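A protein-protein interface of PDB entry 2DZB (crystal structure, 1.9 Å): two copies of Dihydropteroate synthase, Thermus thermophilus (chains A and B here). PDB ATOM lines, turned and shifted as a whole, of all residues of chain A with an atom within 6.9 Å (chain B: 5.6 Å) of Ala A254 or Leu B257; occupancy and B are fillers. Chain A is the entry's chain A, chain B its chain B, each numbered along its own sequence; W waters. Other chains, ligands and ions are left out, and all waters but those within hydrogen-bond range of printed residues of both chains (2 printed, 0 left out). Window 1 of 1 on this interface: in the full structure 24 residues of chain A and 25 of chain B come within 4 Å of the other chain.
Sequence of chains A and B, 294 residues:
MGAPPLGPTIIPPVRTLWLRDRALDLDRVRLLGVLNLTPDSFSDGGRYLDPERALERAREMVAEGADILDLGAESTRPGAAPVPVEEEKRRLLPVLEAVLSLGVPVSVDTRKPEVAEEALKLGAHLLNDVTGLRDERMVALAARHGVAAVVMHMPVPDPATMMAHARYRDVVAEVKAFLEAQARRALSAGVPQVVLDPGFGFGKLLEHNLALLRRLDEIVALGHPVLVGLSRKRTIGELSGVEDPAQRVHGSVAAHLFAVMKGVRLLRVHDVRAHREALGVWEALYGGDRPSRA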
ATOM      1  N   ILE A 236      19.112  39.572  24.775  1.00  0.00           N
ATOM      2  CA  ILE A 236      18.424  38.320  25.077  1.00  0.00           C
ATOM      3  C   ILE A 236      17.257  38.554  26.033  1.00  0.00           C
ATOM      4  O   ILE A 236      16.157  38.045  25.818  1.00  0.00           O
ATOM      5  CB  ILE A 236      19.394  37.296  25.696  1.00  0.00           C
ATOM      6  CG1 ILE A 236      20.553  37.038  24.723  1.00  0.00           C
ATOM      7  CG2 ILE A 236      18.650  36.003  26.030  1.00  0.00           C
ATOM      8  CD1 ILE A 236      20.107  36.639  23.308  1.00  0.00           C
ATOM      9  N   ARG A 248      18.899  33.823  31.663  1.00  0.00           N
ATOM     10  CA  ARG A 248      18.738  33.960  30.214  1.00  0.00           C
ATOM     11  C   ARG A 248      19.342  32.858  29.350  1.00  0.00           C
ATOM     12  O   ARG A 248      19.505  33.047  28.148  1.00  0.00           O
ATOM     13  CB  ARG A 248      19.324  35.305  29.771  1.00  0.00           C
ATOM     14  CG  ARG A 248      18.571  36.500  30.333  1.00  0.00           C
ATOM     15  CD  ARG A 248      19.276  37.828  30.095  1.00  0.00           C
ATOM     16  NE  ARG A 248      18.440  38.925  30.587  1.00  0.00           N
ATOM     17  CZ  ARG A 248      18.861  40.171  30.797  1.00  0.00           C
ATOM     18  NH1 ARG A 248      20.124  40.506  30.565  1.00  0.00           N
ATOM     19  NH2 ARG A 248      18.003  41.090  31.233  1.00  0.00           N
ATOM     20  N   VAL A 249      19.644  31.703  29.933  1.00  0.00           N
ATOM     21  CA  VAL A 249      20.273  30.648  29.145  1.00  0.00           C
ATOM     22  C   VAL A 249      19.500  30.161  27.913  1.00  0.00           C
ATOM     23  O   VAL A 249      20.097  29.973  26.859  1.00  0.00           O
ATOM     24  CB  VAL A 249      20.643  29.423  30.025  1.00  0.00           C
ATOM     25  CG1 VAL A 249      21.335  28.357  29.178  1.00  0.00           C
ATOM     26  CG2 VAL A 249      21.585  29.859  31.128  1.00  0.00           C
ATOM     27  N   HIS A 250      18.188  29.964  28.025  1.00  0.00           N
ATOM     28  CA  HIS A 250      17.424  29.471  26.873  1.00  0.00           C
ATOM     29  C   HIS A 250      17.431  30.454  25.699  1.00  0.00           C
ATOM     30  O   HIS A 250      17.559  30.057  24.539  1.00  0.00           O
ATOM     31  CB  HIS A 250      15.990  29.143  27.297  1.00  0.00           C
ATOM     32  CG  HIS A 250      15.906  28.014  28.279  1.00  0.00           C
ATOM     33  ND1 HIS A 250      16.397  26.755  28.003  1.00  0.00           N
ATOM     34  CD2 HIS A 250      15.433  27.967  29.547  1.00  0.00           C
ATOM     35  CE1 HIS A 250      16.233  25.981  29.064  1.00  0.00           C
ATOM     36  NE2 HIS A 250      15.652  26.692  30.012  1.00  0.00           N
ATOM     37  N   GLY A 251      17.296  31.739  26.001  1.00  0.00           N
ATOM     38  CA  GLY A 251      17.328  32.729  24.940  1.00  0.00           C
ATOM     39  C   GLY A 251      18.729  32.844  24.354  1.00  0.00           C
ATOM     40  O   GLY A 251      18.888  33.026  23.148  1.00  0.00           O
ATOM     41  N   SER A 252      19.752  32.743  25.203  1.00  0.00           N
ATOM     42  CA  SER A 252      21.130  32.832  24.736  1.00  0.00           C
ATOM     43  C   SER A 252      21.471  31.651  23.822  1.00  0.00           C
ATOM     44  O   SER A 252      22.091  31.824  22.769  1.00  0.00           O
ATOM     45  CB  SER A 252      22.095  32.872  25.927  1.00  0.00           C
ATOM     46  OG  SER A 252      21.764  33.936  26.803  1.00  0.00           O
ATOM     47  N   VAL A 253      21.068  30.448  24.221  1.00  0.00           N
ATOM     48  CA  VAL A 253      21.323  29.275  23.390  1.00  0.00           C
ATOM     49  C   VAL A 253      20.645  29.470  22.032  1.00  0.00           C
ATOM     50  O   VAL A 253      21.231  29.184  20.987  1.00  0.00           O
ATOM     51  CB  VAL A 253      20.790  27.980  24.060  1.00  0.00           C
ATOM     52  CG1 VAL A 253      20.821  26.824  23.065  1.00  0.00           C
ATOM     53  CG2 VAL A 253      21.656  27.644  25.279  1.00  0.00           C
ATOM     54  N   ALA A 254      19.417  29.978  22.048  1.00  0.00           N
ATOM     55  CA  ALA A 254      18.681  30.209  20.807  1.00  0.00           C
ATOM     56  C   ALA A 254      19.407  31.205  19.897  1.00  0.00           C
ATOM     57  O   ALA A 254      19.522  30.977  18.690  1.00  0.00           O
ATOM     58  CB  ALA A 254      17.267  30.707  21.114  1.00  0.00           C
ATOM     59  N   ALA A 255      19.891  32.307  20.469  1.00  0.00           N
ATOM     60  CA  ALA A 255      20.606  33.312  19.683  1.00  0.00           C
ATOM     61  C   ALA A 255      21.911  32.727  19.146  1.00  0.00           C
ATOM     62  O   ALA A 255      22.294  32.975  18.003  1.00  0.00           O
ATOM     63  CB  ALA A 255      20.902  34.536  20.544  1.00  0.00           C
ATOM     64  N   HIS A 256      22.593  31.952  19.981  1.00  0.00           N
ATOM     65  CA  HIS A 256      23.855  31.345  19.582  1.00  0.00           C
ATOM     66  C   HIS A 256      23.684  30.299  18.475  1.00  0.00           C
ATOM     67  O   HIS A 256      24.523  30.200  17.581  1.00  0.00           O
ATOM     68  CB  HIS A 256      24.557  30.763  20.816  1.00  0.00           C
ATOM     69  CG  HIS A 256      25.203  31.810  21.674  1.00  0.00           C
ATOM     70  ND1 HIS A 256      25.430  31.641  23.023  1.00  0.00           N
ATOM     71  CD2 HIS A 256      25.686  33.036  21.362  1.00  0.00           C
ATOM     72  CE1 HIS A 256      26.024  32.719  23.505  1.00  0.00           C
ATOM     73  NE2 HIS A 256      26.192  33.580  22.518  1.00  0.00           N
ATOM     74  N   LEU A 257      22.595  29.533  18.515  1.00  0.00           N
ATOM     75  CA  LEU A 257      22.371  28.536  17.470  1.00  0.00           C
ATOM     76  C   LEU A 257      22.102  29.272  16.163  1.00  0.00           C
ATOM     77  O   LEU A 257      22.530  28.844  15.096  1.00  0.00           O
ATOM     78  CB  LEU A 257      21.192  27.625  17.825  1.00  0.00           C
ATOM     79  CG  LEU A 257      21.446  26.660  18.993  1.00  0.00           C
ATOM     80  CD1 LEU A 257      20.240  25.749  19.168  1.00  0.00           C
ATOM     81  CD2 LEU A 257      22.709  25.828  18.713  1.00  0.00           C
ATOM     82  N   PHE A 258      21.397  30.394  16.256  1.00  0.00           N
ATOM     83  CA  PHE A 258      21.117  31.192  15.071  1.00  0.00           C
ATOM     84  C   PHE A 258      22.458  31.660  14.506  1.00  0.00           C
ATOM     85  O   PHE A 258      22.693  31.578  13.298  1.00  0.00           O
ATOM     86  CB  PHE A 258      20.236  32.394  15.436  1.00  0.00           C
ATOM     87  CG  PHE A 258      19.878  33.262  14.260  1.00  0.00           C
ATOM     88  CD1 PHE A 258      18.771  32.961  13.472  1.00  0.00           C
ATOM     89  CD2 PHE A 258      20.657  34.364  13.929  1.00  0.00           C
ATOM     90  CE1 PHE A 258      18.442  33.748  12.365  1.00  0.00           C
ATOM     91  CE2 PHE A 258      20.337  35.158  12.826  1.00  0.00           C
ATOM     92  CZ  PHE A 258      19.228  34.847  12.044  1.00  0.00           C
ATOM     93  N   ALA A 259      23.345  32.136  15.380  1.00  0.00           N
ATOM     94  CA  ALA A 259      24.658  32.602  14.929  1.00  0.00           C
ATOM     95  C   ALA A 259      25.431  31.445  14.283  1.00  0.00           C
ATOM     96  O   ALA A 259      26.106  31.627  13.272  1.00  0.00           O
ATOM     97  CB  ALA A 259      25.451  33.183  16.097  1.00  0.00           C
ATOM     98  N   HIS A 275      25.202  24.777  26.266  1.00  0.00           N
ATOM     99  CA  HIS A 275      25.564  24.881  24.857  1.00  0.00           C
ATOM    100  C   HIS A 275      26.123  23.578  24.281  1.00  0.00           C
ATOM    101  O   HIS A 275      25.846  23.252  23.124  1.00  0.00           O
ATOM    102  CB  HIS A 275      26.549  26.027  24.636  1.00  0.00           C
ATOM    103  CG  HIS A 275      25.928  27.380  24.808  1.00  0.00           C
ATOM    104  ND1 HIS A 275      25.683  27.934  26.046  1.00  0.00           N
ATOM    105  CD2 HIS A 275      25.444  28.262  23.899  1.00  0.00           C
ATOM    106  CE1 HIS A 275      25.078  29.101  25.894  1.00  0.00           C
ATOM    107  NE2 HIS A 275      24.921  29.324  24.600  1.00  0.00           N
ATOM    108  N   TRP A 282      22.121  20.103  17.572  1.00  0.00           N
ATOM    109  CA  TRP A 282      22.167  20.979  16.401  1.00  0.00           C
ATOM    110  C   TRP A 282      23.158  20.548  15.316  1.00  0.00           C
ATOM    111  O   TRP A 282      22.793  20.439  14.131  1.00  0.00           O
ATOM    112  CB  TRP A 282      22.459  22.427  16.848  1.00  0.00           C
ATOM    113  CG  TRP A 282      22.254  23.417  15.751  1.00  0.00           C
ATOM    114  CD1 TRP A 282      23.197  23.880  14.874  1.00  0.00           C
ATOM    115  CD2 TRP A 282      21.011  24.004  15.354  1.00  0.00           C
ATOM    116  NE1 TRP A 282      22.614  24.715  13.953  1.00  0.00           N
ATOM    117  CE2 TRP A 282      21.272  24.808  14.223  1.00  0.00           C
ATOM    118  CE3 TRP A 282      19.698  23.926  15.841  1.00  0.00           C
ATOM    119  CZ2 TRP A 282      20.267  25.533  13.570  1.00  0.00           C
ATOM    120  CZ3 TRP A 282      18.702  24.644  15.191  1.00  0.00           C
ATOM    121  CH2 TRP A 282      18.994  25.438  14.065  1.00  0.00           C
ATOM    122  N   SER B 252      16.468  19.337  23.712  1.00  0.00           N
ATOM    123  CA  SER B 252      15.107  19.343  23.176  1.00  0.00           C
ATOM    124  C   SER B 252      14.789  20.664  22.470  1.00  0.00           C
ATOM    125  O   SER B 252      14.219  20.670  21.382  1.00  0.00           O
ATOM    126  CB  SER B 252      14.087  19.106  24.294  1.00  0.00           C
ATOM    127  OG  SER B 252      14.221  17.800  24.824  1.00  0.00           O
ATOM    128  N   VAL B 253      15.134  21.773  23.114  1.00  0.00           N
ATOM    129  CA  VAL B 253      14.912  23.092  22.529  1.00  0.00           C
ATOM    130  C   VAL B 253      15.667  23.216  21.200  1.00  0.00           C
ATOM    131  O   VAL B 253      15.123  23.739  20.227  1.00  0.00           O
ATOM    132  CB  VAL B 253      15.372  24.212  23.489  1.00  0.00           C
ATOM    133  CG1 VAL B 253      15.445  25.558  22.744  1.00  0.00           C
ATOM    134  CG2 VAL B 253      14.392  24.308  24.670  1.00  0.00           C
ATOM    135  N   ALA B 254      16.907  22.729  21.155  1.00  0.00           N
ATOM    136  CA  ALA B 254      17.701  22.786  19.924  1.00  0.00           C
ATOM    137  C   ALA B 254      17.026  21.995  18.800  1.00  0.00           C
ATOM    138  O   ALA B 254      16.962  22.452  17.656  1.00  0.00           O
ATOM    139  CB  ALA B 254      19.110  22.237  20.173  1.00  0.00           C
ATOM    140  N   ALA B 255      16.532  20.804  19.128  1.00  0.00           N
ATOM    141  CA  ALA B 255      15.855  19.965  18.140  1.00  0.00           C
ATOM    142  C   ALA B 255      14.606  20.657  17.610  1.00  0.00           C
ATOM    143  O   ALA B 255      14.352  20.686  16.402  1.00  0.00           O
ATOM    144  CB  ALA B 255      15.471  18.627  18.764  1.00  0.00           C
ATOM    145  N   HIS B 256      13.817  21.204  18.526  1.00  0.00           N
ATOM    146  CA  HIS B 256      12.602  21.896  18.151  1.00  0.00           C
ATOM    147  C   HIS B 256      12.860  23.154  17.326  1.00  0.00           C
ATOM    148  O   HIS B 256      12.090  23.458  16.426  1.00  0.00           O
ATOM    149  CB  HIS B 256      11.796  22.208  19.407  1.00  0.00           C
ATOM    150  CG  HIS B 256      11.123  21.003  19.986  1.00  0.00           C
ATOM    151  ND1 HIS B 256      10.808  20.891  21.322  1.00  0.00           N
ATOM    152  CD2 HIS B 256      10.696  19.859  19.399  1.00  0.00           C
ATOM    153  CE1 HIS B 256      10.214  19.729  21.535  1.00  0.00           C
ATOM    154  NE2 HIS B 256      10.134  19.084  20.385  1.00  0.00           N
ATOM    155  N   LEU B 257      13.935  23.884  17.620  1.00  0.00           N
ATOM    156  CA  LEU B 257      14.235  25.081  16.828  1.00  0.00           C
ATOM    157  C   LEU B 257      14.592  24.649  15.408  1.00  0.00           C
ATOM    158  O   LEU B 257      14.250  25.330  14.437  1.00  0.00           O
ATOM    159  CB  LEU B 257      15.392  25.881  17.451  1.00  0.00           C
ATOM    160  CG  LEU B 257      15.020  26.530  18.792  1.00  0.00           C
ATOM    161  CD1 LEU B 257      16.211  27.278  19.384  1.00  0.00           C
ATOM    162  CD2 LEU B 257      13.830  27.476  18.571  1.00  0.00           C
ATOM    163  N   PHE B 258      15.281  23.518  15.284  1.00  0.00           N
ATOM    164  CA  PHE B 258      15.634  23.008  13.965  1.00  0.00           C
ATOM    165  C   PHE B 258      14.340  22.676  13.222  1.00  0.00           C
ATOM    166  O   PHE B 258      14.202  22.976  12.035  1.00  0.00           O
ATOM    167  CB  PHE B 258      16.529  21.758  14.080  1.00  0.00           C
ATOM    168  CG  PHE B 258      16.973  21.195  12.744  1.00  0.00           C
ATOM    169  CD1 PHE B 258      18.144  21.649  12.139  1.00  0.00           C
ATOM    170  CD2 PHE B 258      16.219  20.223  12.095  1.00  0.00           C
ATOM    171  CE1 PHE B 258      18.562  21.141  10.894  1.00  0.00           C
ATOM    172  CE2 PHE B 258      16.618  19.705  10.854  1.00  0.00           C
ATOM    173  CZ  PHE B 258      17.797  20.166  10.253  1.00  0.00           C
ATOM    174  N   ALA B 259      13.392  22.059  13.922  1.00  0.00           N
ATOM    175  CA  ALA B 259      12.102  21.709  13.317  1.00  0.00           C
ATOM    176  C   ALA B 259      11.384  22.987  12.895  1.00  0.00           C
ATOM    177  O   ALA B 259      10.767  23.044  11.834  1.00  0.00           O
ATOM    178  CB  ALA B 259      11.233  20.945  14.309  1.00  0.00           C
ATOM    179  N   VAL B 260      11.463  24.015  13.733  1.00  0.00           N
ATOM    180  CA  VAL B 260      10.804  25.275  13.410  1.00  0.00           C
ATOM    181  C   VAL B 260      11.398  25.839  12.124  1.00  0.00           C
ATOM    182  O   VAL B 260      10.676  26.334  11.251  1.00  0.00           O
ATOM    183  CB  VAL B 260      10.949  26.289  14.567  1.00  0.00           C
ATOM    184  CG1 VAL B 260      10.494  27.683  14.114  1.00  0.00           C
ATOM    185  CG2 VAL B 260      10.100  25.836  15.736  1.00  0.00           C
ATOM    186  N   MET B 261      12.716  25.749  12.002  1.00  0.00           N
ATOM    187  CA  MET B 261      13.407  26.228  10.813  1.00  0.00           C
ATOM    188  C   MET B 261      12.950  25.452   9.569  1.00  0.00           C
ATOM    189  O   MET B 261      12.949  25.984   8.459  1.00  0.00           O
ATOM    190  CB  MET B 261      14.912  26.074  11.002  1.00  0.00           C
ATOM    191  CG  MET B 261      15.727  26.567   9.831  1.00  0.00           C
ATOM    192  SD  MET B 261      17.471  26.436  10.188  1.00  0.00           S
ATOM    193  CE  MET B 261      17.761  24.673   9.815  1.00  0.00           C
ATOM    194  N   LYS B 262      12.565  24.196   9.766  1.00  0.00           N
ATOM    195  CA  LYS B 262      12.094  23.336   8.676  1.00  0.00           C
ATOM    196  C   LYS B 262      10.628  23.590   8.319  1.00  0.00           C
ATOM    197  O   LYS B 262      10.088  22.981   7.384  1.00  0.00           O
ATOM    198  CB  LYS B 262      12.282  21.861   9.056  1.00  0.00           C
ATOM    199  CG  LYS B 262      13.719  21.387   8.971  1.00  0.00           C
ATOM    200  CD  LYS B 262      14.161  21.313   7.518  1.00  0.00           C
ATOM    201  CE  LYS B 262      15.558  20.745   7.385  1.00  0.00           C
ATOM    202  NZ  LYS B 262      15.846  20.337   5.979  1.00  0.00           N
ATOM    203  N   GLU B 277      10.818  31.211  25.862  1.00  0.00           N
ATOM    204  CA  GLU B 277      11.978  32.101  25.867  1.00  0.00           C
ATOM    205  C   GLU B 277      12.841  31.924  24.622  1.00  0.00           C
ATOM    206  O   GLU B 277      13.265  32.909  24.006  1.00  0.00           O
ATOM    207  CB  GLU B 277      12.837  31.861  27.118  1.00  0.00           C
ATOM    208  CG  GLU B 277      12.114  32.123  28.434  1.00  0.00           C
ATOM    209  CD  GLU B 277      12.984  31.834  29.646  1.00  0.00           C
ATOM    210  OE1 GLU B 277      14.171  31.508  29.454  1.00  0.00           O
ATOM    211  OE2 GLU B 277      12.486  31.932  30.787  1.00  0.00           O
ATOM    212  N   ALA B 278      13.109  30.673  24.253  1.00  0.00           N
ATOM    213  CA  ALA B 278      13.930  30.409  23.073  1.00  0.00           C
ATOM    214  C   ALA B 278      13.256  30.921  21.799  1.00  0.00           C
ATOM    215  O   ALA B 278      13.915  31.512  20.953  1.00  0.00           O
ATOM    216  CB  ALA B 278      14.230  28.899  22.941  1.00  0.00           C
ATOM    217  N   LEU B 279      11.950  30.696  21.668  1.00  0.00           N
ATOM    218  CA  LEU B 279      11.212  31.139  20.484  1.00  0.00           C
ATOM    219  C   LEU B 279      11.128  32.665  20.418  1.00  0.00           C
ATOM    220  O   LEU B 279      11.071  33.243  19.334  1.00  0.00           O
ATOM    221  CB  LEU B 279       9.802  30.524  20.467  1.00  0.00           C
ATOM    222  CG  LEU B 279       9.724  29.025  20.115  1.00  0.00           C
ATOM    223  CD1 LEU B 279       8.346  28.473  20.439  1.00  0.00           C
ATOM    224  CD2 LEU B 279      10.053  28.846  18.633  1.00  0.00           C
ATOM    225  N   VAL B 281      13.431  34.724  21.071  1.00  0.00           N
ATOM    226  CA  VAL B 281      14.664  35.112  20.394  1.00  0.00           C
ATOM    227  C   VAL B 281      14.644  34.620  18.947  1.00  0.00           C
ATOM    228  O   VAL B 281      14.778  35.408  18.015  1.00  0.00           O
ATOM    229  CB  VAL B 281      15.914  34.517  21.087  1.00  0.00           C
ATOM    230  CG1 VAL B 281      17.148  34.742  20.222  1.00  0.00           C
ATOM    231  CG2 VAL B 281      16.122  35.163  22.449  1.00  0.00           C
ATOM    232  N   TRP B 282      14.467  33.311  18.766  1.00  0.00           N
ATOM    233  CA  TRP B 282      14.461  32.724  17.428  1.00  0.00           C
ATOM    234  C   TRP B 282      13.520  33.381  16.417  1.00  0.00           C
ATOM    235  O   TRP B 282      13.925  33.693  15.292  1.00  0.00           O
ATOM    236  CB  TRP B 282      14.140  31.229  17.505  1.00  0.00           C
ATOM    237  CG  TRP B 282      14.369  30.530  16.219  1.00  0.00           C
ATOM    238  CD1 TRP B 282      13.453  30.288  15.232  1.00  0.00           C
ATOM    239  CD2 TRP B 282      15.614  30.013  15.748  1.00  0.00           C
ATOM    240  NE1 TRP B 282      14.058  29.646  14.175  1.00  0.00           N
ATOM    241  CE2 TRP B 282      15.385  29.466  14.468  1.00  0.00           C
ATOM    242  CE3 TRP B 282      16.906  29.963  16.286  1.00  0.00           C
ATOM    243  CZ2 TRP B 282      16.400  28.872  13.715  1.00  0.00           C
ATOM    244  CZ3 TRP B 282      17.917  29.374  15.538  1.00  0.00           C
ATOM    245  CH2 TRP B 282      17.656  28.836  14.266  1.00  0.00           C
ATOM    246  N   LEU B 285      14.621  36.727  15.208  1.00  0.00           N
ATOM    247  CA  LEU B 285      15.802  36.705  14.349  1.00  0.00           C
ATOM    248  C   LEU B 285      15.569  36.064  12.990  1.00  0.00           C
ATOM    249  O   LEU B 285      16.042  36.560  11.970  1.00  0.00           O
ATOM    250  CB  LEU B 285      16.946  35.961  15.038  1.00  0.00           C
ATOM    251  CG  LEU B 285      17.377  36.410  16.431  1.00  0.00           C
ATOM    252  CD1 LEU B 285      18.604  35.615  16.838  1.00  0.00           C
ATOM    253  CD2 LEU B 285      17.682  37.905  16.437  1.00  0.00           C
HETATM  254  O   HOH W   1      16.168  33.736  27.922  1.00  0.00           O
HETATM  255  O   HOH W   2      16.398  30.933  30.263  1.00  0.00           O
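Among the printed residues, merely in contact across the chains: Ala A254 with Ala B278, Gly A251 with Val B281, Trp A282 with Ala B254, Trp A282 with Phe B258, Phe A258 with Leu B285, Trp A282 with Trp B282, Ala A255 with Val B281, His A250 with Glu B277, Ala A254 with Trp B282, Phe A258 with Trp B282, Leu A257 with Ala B254, His A250 with Ala B278 and Ala A254 with Leu B257.
Printed residues of chain B within 4 Å of Ala A254: Leu B257 (3.98 Å), Ala B278 (3.5 Å) and Trp B282 (3.7 Å). Of the printed residues of chain A, Leu B257 touches Ala A254 (3.98 Å). Of the printed residues of chain B, Leu A257 touches Ala B254 (3.8 Å). Of the printed residues of chain A, Trp B282 touches Ala A254, Phe A258 and Trp A282. Arg A248 touches none of the printed residues of chain B. The nearest printed residue of chain B that does not touch Ala A254 is Val B281 (4.04 Å). The nearest printed residue of chain B that does not touch Gly A251 is Glu B277 (4.2 Å).
Along chain A the printed residues that touch a printed residue of chain B span positions 250 to 282. Printed residues of chain B that touch a printed residue of chain A: Ala B254, Leu B257, Phe B258, Glu B277, Ala B278, Val B281, Trp B282 and Leu B285. Hydrophobic or aromatic side chains of chain B that line the printed part of chain A: Ala B254, Leu B257, Phe B258, Ala B278, Val B281, Trp B282 and Leu B285.
Ala A254 touches Leu B257, and with the chains exchanged Leu A257 touches Ala B254. Ala A254 touches Trp B282, and with the chains exchanged Trp A282 touches Ala B254. Phe A258 touches Trp B282, and with the chains exchanged Trp A282 touches Phe B258. Trp B282 touches its own counterpart, Trp A282. Positions printed for both chains: 252, 253, 254, 255, 256, 257, 258, 259 and 282.
Water W2 lies within hydrogen-bond range of the side-chain carboxylate of Glu B277, the backbone NH of His A250 and the backbone NH of Val A249. Water W1 lies within hydrogen-bond range of N of Gly A251 (3.0 Å), OE1 of Glu B277 (3.4 Å) and O of Arg A248 (3.4 Å).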
